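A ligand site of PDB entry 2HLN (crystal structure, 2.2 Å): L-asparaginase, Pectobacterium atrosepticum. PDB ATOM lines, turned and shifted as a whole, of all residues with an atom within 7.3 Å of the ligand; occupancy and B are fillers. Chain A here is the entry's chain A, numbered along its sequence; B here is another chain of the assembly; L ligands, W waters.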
ATOM      1  N   GLY A  13       7.050  14.949  19.656  1.00  0.00           N
ATOM      2  CA  GLY A  13       7.091  16.370  19.977  1.00  0.00           C
ATOM      3  C   GLY A  13       6.315  16.688  21.239  1.00  0.00           C
ATOM      4  O   GLY A  13       6.216  15.844  22.134  1.00  0.00           O
ATOM      5  N   GLY A  14       5.761  17.895  21.300  1.00  0.00           N
ATOM      6  CA  GLY A  14       4.991  18.326  22.467  1.00  0.00           C
ATOM      7  C   GLY A  14       5.867  19.023  23.498  1.00  0.00           C
ATOM      8  O   GLY A  14       7.093  18.922  23.455  1.00  0.00           O
ATOM      9  N   THR A  15       5.234  19.709  24.444  1.00  0.00           N
ATOM     10  CA  THR A  15       5.970  20.437  25.472  1.00  0.00           C
ATOM     11  C   THR A  15       6.469  19.523  26.592  1.00  0.00           C
ATOM     12  O   THR A  15       7.255  19.946  27.445  1.00  0.00           O
ATOM     13  CB  THR A  15       5.148  21.610  26.071  1.00  0.00           C
ATOM     14  OG1 THR A  15       6.016  22.488  26.800  1.00  0.00           O
ATOM     15  CG2 THR A  15       4.051  21.089  26.998  1.00  0.00           C
ATOM     16  N   ILE A  16       6.009  18.273  26.583  1.00  0.00           N
ATOM     17  CA  ILE A  16       6.424  17.284  27.579  1.00  0.00           C
ATOM     18  C   ILE A  16       7.924  16.998  27.454  1.00  0.00           C
ATOM     19  O   ILE A  16       8.571  16.610  28.429  1.00  0.00           O
ATOM     20  CB  ILE A  16       5.593  15.969  27.466  1.00  0.00           C
ATOM     21  CG1 ILE A  16       5.903  15.024  28.635  1.00  0.00           C
ATOM     22  CG2 ILE A  16       5.798  15.303  26.110  1.00  0.00           C
ATOM     23  CD1 ILE A  16       5.079  13.751  28.643  1.00  0.00           C
ATOM     24  N   ALA A  17       8.472  17.233  26.260  1.00  0.00           N
ATOM     25  CA  ALA A  17       9.883  17.021  25.997  1.00  0.00           C
ATOM     26  C   ALA A  17      10.646  18.339  26.072  1.00  0.00           C
ATOM     27  O   ALA A  17      10.771  18.936  27.138  1.00  0.00           O
ATOM     28  CB  ALA A  17      10.070  16.377  24.630  1.00  0.00           C
ATOM     29  N   ILE A  60       7.654  17.818  16.294  1.00  0.00           N
ATOM     30  CA  ILE A  60       6.810  18.951  15.968  1.00  0.00           C
ATOM     31  C   ILE A  60       5.746  19.165  17.038  1.00  0.00           C
ATOM     32  O   ILE A  60       5.491  18.285  17.864  1.00  0.00           O
ATOM     33  CB  ILE A  60       6.080  18.745  14.617  1.00  0.00           C
ATOM     34  CG1 ILE A  60       5.296  17.426  14.635  1.00  0.00           C
ATOM     35  CG2 ILE A  60       7.073  18.764  13.452  1.00  0.00           C
ATOM     36  CD1 ILE A  60       4.531  17.140  13.384  1.00  0.00           C
ATOM     37  N   GLY A  61       5.118  20.344  17.017  1.00  0.00           N
ATOM     38  CA  GLY A  61       4.030  20.632  17.930  1.00  0.00           C
ATOM     39  C   GLY A  61       2.798  19.911  17.412  1.00  0.00           C
ATOM     40  O   GLY A  61       2.643  19.749  16.202  1.00  0.00           O
ATOM     41  N   SER A  62       1.933  19.495  18.329  1.00  0.00           N
ATOM     42  CA  SER A  62       0.724  18.748  17.974  1.00  0.00           C
ATOM     43  C   SER A  62      -0.171  19.461  16.959  1.00  0.00           C
ATOM     44  O   SER A  62      -0.856  18.819  16.165  1.00  0.00           O
ATOM     45  CB  SER A  62      -0.083  18.404  19.223  1.00  0.00           C
ATOM     46  OG  SER A  62      -1.211  17.615  18.919  1.00  0.00           O
ATOM     47  N   GLU A  63      -0.164  20.795  16.999  1.00  0.00           N
ATOM     48  CA  GLU A  63      -0.954  21.594  16.069  1.00  0.00           C
ATOM     49  C   GLU A  63      -0.558  21.321  14.618  1.00  0.00           C
ATOM     50  O   GLU A  63      -1.355  21.483  13.703  1.00  0.00           O
ATOM     51  CB  GLU A  63      -0.838  23.097  16.400  1.00  0.00           C
ATOM     52  CG  GLU A  63       0.543  23.737  16.145  1.00  0.00           C
ATOM     53  CD  GLU A  63       1.583  23.389  17.198  1.00  0.00           C
ATOM     54  OE1 GLU A  63       1.252  22.670  18.166  1.00  0.00           O
ATOM     55  OE2 GLU A  63       2.737  23.850  17.064  1.00  0.00           O
ATOM     56  N   ASN A  64       0.684  20.894  14.421  1.00  0.00           N
ATOM     57  CA  ASN A  64       1.205  20.578  13.094  1.00  0.00           C
ATOM     58  C   ASN A  64       1.316  19.089  12.789  1.00  0.00           C
ATOM     59  O   ASN A  64       1.975  18.700  11.817  1.00  0.00           O
ATOM     60  CB  ASN A  64       2.533  21.291  12.835  1.00  0.00           C
ATOM     61  CG  ASN A  64       2.335  22.733  12.407  1.00  0.00           C
ATOM     62  OD1 ASN A  64       1.409  23.046  11.660  1.00  0.00           O
ATOM     63  ND2 ASN A  64       3.240  23.611  12.833  1.00  0.00           N
ATOM     64  N   HIS A  93       3.362  13.057  22.996  1.00  0.00           N
ATOM     65  CA  HIS A  93       2.670  13.794  21.963  1.00  0.00           C
ATOM     66  C   HIS A  93       2.146  15.088  22.576  1.00  0.00           C
ATOM     67  O   HIS A  93       2.036  15.194  23.791  1.00  0.00           O
ATOM     68  CB  HIS A  93       1.493  12.930  21.503  1.00  0.00           C
ATOM     69  CG  HIS A  93       0.790  13.413  20.275  1.00  0.00           C
ATOM     70  ND1 HIS A  93      -0.249  14.321  20.327  1.00  0.00           N
ATOM     71  CD2 HIS A  93       0.874  13.016  18.984  1.00  0.00           C
ATOM     72  CE1 HIS A  93      -0.722  14.511  19.111  1.00  0.00           C
ATOM     73  NE2 HIS A  93      -0.060  13.729  18.272  1.00  0.00           N
ATOM     74  N   GLY A  94       1.866  16.088  21.738  1.00  0.00           N
ATOM     75  CA  GLY A  94       1.298  17.344  22.230  1.00  0.00           C
ATOM     76  C   GLY A  94      -0.167  17.162  22.562  1.00  0.00           C
ATOM     77  O   GLY A  94      -0.789  16.186  22.144  1.00  0.00           O
ATOM     78  N   THR A  95      -0.751  18.108  23.297  1.00  0.00           N
ATOM     79  CA  THR A  95      -2.148  18.015  23.714  1.00  0.00           C
ATOM     80  C   THR A  95      -3.166  18.545  22.693  1.00  0.00           C
ATOM     81  O   THR A  95      -4.300  18.060  22.637  1.00  0.00           O
ATOM     82  CB  THR A  95      -2.415  18.726  25.057  1.00  0.00           C
ATOM     83  OG1 THR A  95      -2.235  20.145  24.892  1.00  0.00           O
ATOM     84  CG2 THR A  95      -1.474  18.220  26.134  1.00  0.00           C
ATOM     85  N   ASP A  96      -2.763  19.531  21.897  1.00  0.00           N
ATOM     86  CA  ASP A  96      -3.661  20.188  20.929  1.00  0.00           C
ATOM     87  C   ASP A  96      -4.445  19.286  19.967  1.00  0.00           C
ATOM     88  O   ASP A  96      -5.608  19.576  19.659  1.00  0.00           O
ATOM     89  CB  ASP A  96      -2.958  21.314  20.184  1.00  0.00           C
ATOM     90  CG  ASP A  96      -2.536  22.440  21.105  1.00  0.00           C
ATOM     91  OD1 ASP A  96      -3.070  22.532  22.232  1.00  0.00           O
ATOM     92  OD2 ASP A  96      -1.661  23.239  20.712  1.00  0.00           O
ATOM     93  N   THR A  97      -3.799  18.248  19.463  1.00  0.00           N
ATOM     94  CA  THR A  97      -4.487  17.296  18.582  1.00  0.00           C
ATOM     95  C   THR A  97      -4.417  15.878  19.145  1.00  0.00           C
ATOM     96  O   THR A  97      -4.326  14.905  18.404  1.00  0.00           O
ATOM     97  CB  THR A  97      -3.947  17.308  17.143  1.00  0.00           C
ATOM     98  OG1 THR A  97      -2.538  17.029  17.133  1.00  0.00           O
ATOM     99  CG2 THR A  97      -4.201  18.648  16.483  1.00  0.00           C
ATOM    100  N   LEU A  98      -4.475  15.780  20.473  1.00  0.00           N
ATOM    101  CA  LEU A  98      -4.464  14.492  21.135  1.00  0.00           C
ATOM    102  C   LEU A  98      -5.862  13.854  21.046  1.00  0.00           C
ATOM    103  O   LEU A  98      -6.110  12.788  21.604  1.00  0.00           O
ATOM    104  CB  LEU A  98      -4.002  14.649  22.589  1.00  0.00           C
ATOM    105  CG  LEU A  98      -3.522  13.387  23.326  1.00  0.00           C
ATOM    106  CD1 LEU A  98      -2.388  12.720  22.570  1.00  0.00           C
ATOM    107  CD2 LEU A  98      -3.082  13.721  24.747  1.00  0.00           C
ATOM    108  N   ALA A 119       0.982  13.277  27.406  1.00  0.00           N
ATOM    109  CA  ALA A 119       1.254  14.676  27.105  1.00  0.00           C
ATOM    110  C   ALA A 119       1.350  15.508  28.374  1.00  0.00           C
ATOM    111  O   ALA A 119       1.162  15.000  29.484  1.00  0.00           O
ATOM    112  CB  ALA A 119       0.183  15.220  26.183  1.00  0.00           C
ATOM    113  N   ALA A 120       1.648  16.789  28.214  1.00  0.00           N
ATOM    114  CA  ALA A 120       1.742  17.715  29.341  1.00  0.00           C
ATOM    115  C   ALA A 120       1.085  19.036  28.993  1.00  0.00           C
ATOM    116  O   ALA A 120       1.220  19.540  27.877  1.00  0.00           O
ATOM    117  CB  ALA A 120       3.215  17.929  29.725  1.00  0.00           C
ATOM    118  N   MET A 121       0.331  19.599  29.949  1.00  0.00           N
ATOM    119  CA  MET A 121      -0.337  20.879  29.752  1.00  0.00           C
ATOM    120  C   MET A 121       0.543  22.065  30.119  1.00  0.00           C
ATOM    121  O   MET A 121       0.253  23.200  29.754  1.00  0.00           O
ATOM    122  CB  MET A 121      -1.665  20.927  30.509  1.00  0.00           C
ATOM    123  CG  MET A 121      -2.769  20.122  29.867  1.00  0.00           C
ATOM    124  SD  MET A 121      -3.189  20.743  28.215  1.00  0.00           S
ATOM    125  CE  MET A 121      -3.918  22.333  28.608  1.00  0.00           C
ATOM    126  N   ARG A 122       1.628  21.785  30.828  1.00  0.00           N
ATOM    127  CA  ARG A 122       2.586  22.811  31.243  1.00  0.00           C
ATOM    128  C   ARG A 122       3.982  22.486  30.744  1.00  0.00           C
ATOM    129  O   ARG A 122       4.369  21.317  30.682  1.00  0.00           O
ATOM    130  CB  ARG A 122       2.625  22.927  32.771  1.00  0.00           C
ATOM    131  CG  ARG A 122       1.364  23.488  33.404  1.00  0.00           C
ATOM    132  CD  ARG A 122       1.486  23.481  34.919  1.00  0.00           C
ATOM    133  NE  ARG A 122       0.256  23.938  35.561  1.00  0.00           N
ATOM    134  CZ  ARG A 122       0.028  23.872  36.872  1.00  0.00           C
ATOM    135  NH1 ARG A 122       0.934  23.328  37.675  1.00  0.00           N
ATOM    136  NH2 ARG A 122      -1.108  24.314  37.370  1.00  0.00           N
ATOM    137  N   PRO A 123       4.757  23.534  30.380  1.00  0.00           N
ATOM    138  CA  PRO A 123       6.137  23.349  29.942  1.00  0.00           C
ATOM    139  C   PRO A 123       6.960  22.647  31.018  1.00  0.00           C
ATOM    140  O   PRO A 123       6.667  22.793  32.209  1.00  0.00           O
ATOM    141  CB  PRO A 123       6.637  24.791  29.756  1.00  0.00           C
ATOM    142  CG  PRO A 123       5.415  25.584  29.498  1.00  0.00           C
ATOM    143  CD  PRO A 123       4.336  24.950  30.321  1.00  0.00           C
ATOM    144  N   LYS A 168      -9.764  16.834  24.548  1.00  0.00           N
ATOM    145  CA  LYS A 168      -9.353  17.996  25.326  1.00  0.00           C
ATOM    146  C   LYS A 168     -10.592  18.885  25.481  1.00  0.00           C
ATOM    147  O   LYS A 168     -11.046  19.499  24.519  1.00  0.00           O
ATOM    148  CB  LYS A 168      -8.219  18.729  24.580  1.00  0.00           C
ATOM    149  CG  LYS A 168      -7.534  19.843  25.360  1.00  0.00           C
ATOM    150  CD  LYS A 168      -6.312  20.355  24.613  1.00  0.00           C
ATOM    151  CE  LYS A 168      -5.618  21.473  25.397  1.00  0.00           C
ATOM    152  NZ  LYS A 168      -4.354  21.926  24.734  1.00  0.00           N
ATOM    153  N   PHE A 177      -8.460  16.734  29.835  1.00  0.00           N
ATOM    154  CA  PHE A 177      -8.904  15.527  29.145  1.00  0.00           C
ATOM    155  C   PHE A 177     -10.008  14.754  29.857  1.00  0.00           C
ATOM    156  O   PHE A 177      -9.765  14.059  30.835  1.00  0.00           O
ATOM    157  CB  PHE A 177      -7.731  14.634  28.759  1.00  0.00           C
ATOM    158  CG  PHE A 177      -6.885  15.205  27.666  1.00  0.00           C
ATOM    159  CD1 PHE A 177      -7.194  14.944  26.336  1.00  0.00           C
ATOM    160  CD2 PHE A 177      -5.815  16.031  27.954  1.00  0.00           C
ATOM    161  CE1 PHE A 177      -6.431  15.487  25.314  1.00  0.00           C
ATOM    162  CE2 PHE A 177      -5.056  16.582  26.937  1.00  0.00           C
ATOM    163  CZ  PHE A 177      -5.358  16.314  25.626  1.00  0.00           C
ATOM    164  N   MET B 250      -7.274  24.495  17.783  1.00  0.00           N
ATOM    165  CA  MET B 250      -6.850  23.320  18.534  1.00  0.00           C
ATOM    166  C   MET B 250      -6.274  23.780  19.867  1.00  0.00           C
ATOM    167  O   MET B 250      -5.431  24.669  19.905  1.00  0.00           O
ATOM    168  CB  MET B 250      -5.771  22.570  17.746  1.00  0.00           C
ATOM    169  CG  MET B 250      -6.248  22.012  16.419  1.00  0.00           C
ATOM    170  SD  MET B 250      -4.906  21.620  15.283  1.00  0.00           S
ATOM    171  CE  MET B 250      -4.322  23.264  14.863  1.00  0.00           C
ATOM    172  N   GLY B 251      -6.747  23.178  20.956  1.00  0.00           N
ATOM    173  CA  GLY B 251      -6.296  23.552  22.297  1.00  0.00           C
ATOM    174  C   GLY B 251      -6.585  25.014  22.584  1.00  0.00           C
ATOM    175  O   GLY B 251      -7.702  25.486  22.405  1.00  0.00           O
ATOM    176  N   ALA B 252      -5.556  25.747  23.011  1.00  0.00           N
ATOM    177  CA  ALA B 252      -5.707  27.164  23.327  1.00  0.00           C
ATOM    178  C   ALA B 252      -5.479  28.055  22.105  1.00  0.00           C
ATOM    179  O   ALA B 252      -4.490  28.790  22.022  1.00  0.00           O
ATOM    180  CB  ALA B 252      -4.764  27.557  24.457  1.00  0.00           C
ATOM    181  N   SER B 254      -4.406  27.419  19.239  1.00  0.00           N
ATOM    182  CA  SER B 254      -3.176  27.125  18.521  1.00  0.00           C
ATOM    183  C   SER B 254      -3.388  26.959  17.021  1.00  0.00           C
ATOM    184  O   SER B 254      -4.317  26.266  16.591  1.00  0.00           O
ATOM    185  CB  SER B 254      -2.494  25.877  19.093  1.00  0.00           C
ATOM    186  OG  SER B 254      -2.205  26.050  20.462  1.00  0.00           O
ATOM    187  N   VAL B 255      -2.527  27.593  16.229  1.00  0.00           N
ATOM    188  CA  VAL B 255      -2.632  27.534  14.780  1.00  0.00           C
ATOM    189  C   VAL B 255      -1.591  26.607  14.162  1.00  0.00           C
ATOM    190  O   VAL B 255      -0.474  26.491  14.669  1.00  0.00           O
ATOM    191  CB  VAL B 255      -2.484  28.943  14.134  1.00  0.00           C
ATOM    192  CG1 VAL B 255      -3.613  29.846  14.577  1.00  0.00           C
ATOM    193  CG2 VAL B 255      -1.133  29.563  14.479  1.00  0.00           C
ATOM    194  N   GLN B 290       1.938  34.436  17.990  1.00  0.00           N
ATOM    195  CA  GLN B 290       0.871  33.995  17.104  1.00  0.00           C
ATOM    196  C   GLN B 290       0.037  35.173  16.596  1.00  0.00           C
ATOM    197  O   GLN B 290      -0.076  36.196  17.271  1.00  0.00           O
ATOM    198  CB  GLN B 290      -0.030  32.965  17.801  1.00  0.00           C
ATOM    199  CG  GLN B 290       0.619  31.598  17.966  1.00  0.00           C
ATOM    200  CD  GLN B 290      -0.288  30.600  18.670  1.00  0.00           C
ATOM    201  OE1 GLN B 290      -0.419  29.454  18.253  1.00  0.00           O
ATOM    202  NE2 GLN B 290      -0.942  31.055  19.742  1.00  0.00           N
HETATM  203  N1  LIG L   1       0.858  23.514  20.704  1.00  0.00           N
HETATM  204  C1  LIG L   1       1.575  22.544  21.570  1.00  0.00           C
HETATM  205  C2  LIG L   1       1.285  21.124  21.172  1.00  0.00           C
HETATM  206  O1  LIG L   1       0.129  20.708  21.157  1.00  0.00           O
HETATM  207  C3  LIG L   1       1.171  22.760  23.020  1.00  0.00           C
HETATM  208  C4  LIG L   1       2.116  22.036  23.973  1.00  0.00           C
HETATM  209  C5  LIG L   1       1.597  20.648  24.275  1.00  0.00           C
HETATM  210  O2  LIG L   1       0.372  20.474  24.406  1.00  0.00           O
HETATM  211  O3  LIG L   1       2.430  19.714  24.380  1.00  0.00           O
HETATM  212  O4  LIG L   1       2.197  20.342  20.895  1.00  0.00           O
HETATM  213  O   HOH W   1       1.901  25.982  21.681  1.00  0.00           O
HETATM  214  O   HOH W   2       2.846  17.397  25.565  1.00  0.00           O
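CA of Gly 14 touches O3 of the ligand, at 3.5 Å.
Gly 61 touches the ligand (CA to O4, 3.5 Å).
Gly 94 touches the ligand (CA to O3, 3.4 Å).
Ala 120 touches the ligand (O to O2, 3.7 Å).
Ser 254 of chain B touches the ligand (OG to N1, 3.98 Å).
Ten residues have an atom within 4 Å of the ligand: Gly 14, Thr 15, Gly 61, Ser 62, Glu 63, Gly 94, Thr 95, Asp 96, Ala 120 and Ser 254 of chain B.
Water W2 lies within hydrogen-bond range of an oxygen (O3) of the ligand (2.6 Å), the backbone carbonyl oxygen (O) of His 93 (2.9 Å), the backbone NH (N) of Ala 120 (3.0 Å) and the backbone NH (N) of Ile 16 (3.4 Å).
The side-chain hydroxyl (OG1) of Thr 95 sits at hydrogen-bond distance from an oxygen (O2) of the ligand, 2.7 Å away.
The side-chain carboxylate (OD2) of Asp 96 is in salt-bridge range of a nitrogen (N1) of the ligand.
O4 of the ligand sits at hydrogen-bond distance from N of Ser 62 (2.7 Å).
OE1 of Glu 63 is in salt-bridge range of N1 of the ligand.
The backbone NH (N) of Thr 15 lies within hydrogen-bond range of an oxygen (O3) of the ligand, 2.8 Å away.
O1 of the ligand sits close to N of Asp 96 (3.2 Å).
N of Thr 95 lies within hydrogen-bond range of O2 of the ligand, at 2.8 Å.
The side-chain hydroxyl (OG1) of Thr 95 sits at hydrogen-bond distance from the side-chain sulfur (SD) of Met 121 (3.5 Å).
OG1 of Thr 97 lies within hydrogen-bond range of O of Ser 62 (2.6 Å).
NZ of Lys 168 sits at hydrogen-bond distance from OG1 of Thr 95 (2.8 Å).
The backbone NH (N) of Gly 14 is in hydrogen-bond range of the backbone carbonyl oxygen (O) of Ile 60 (3.5 Å).
The side-chain carboxylate (OD1) of Asp 96 lies within salt-bridge range of the side-chain amino group (NZ) of Lys 168, at 2.9 Å.
The side-chain carboxylate (OD2) of Asp 96 is in hydrogen-bond range of the side-chain hydroxyl (OG) of Ser 254 of chain B, at 2.9 Å.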
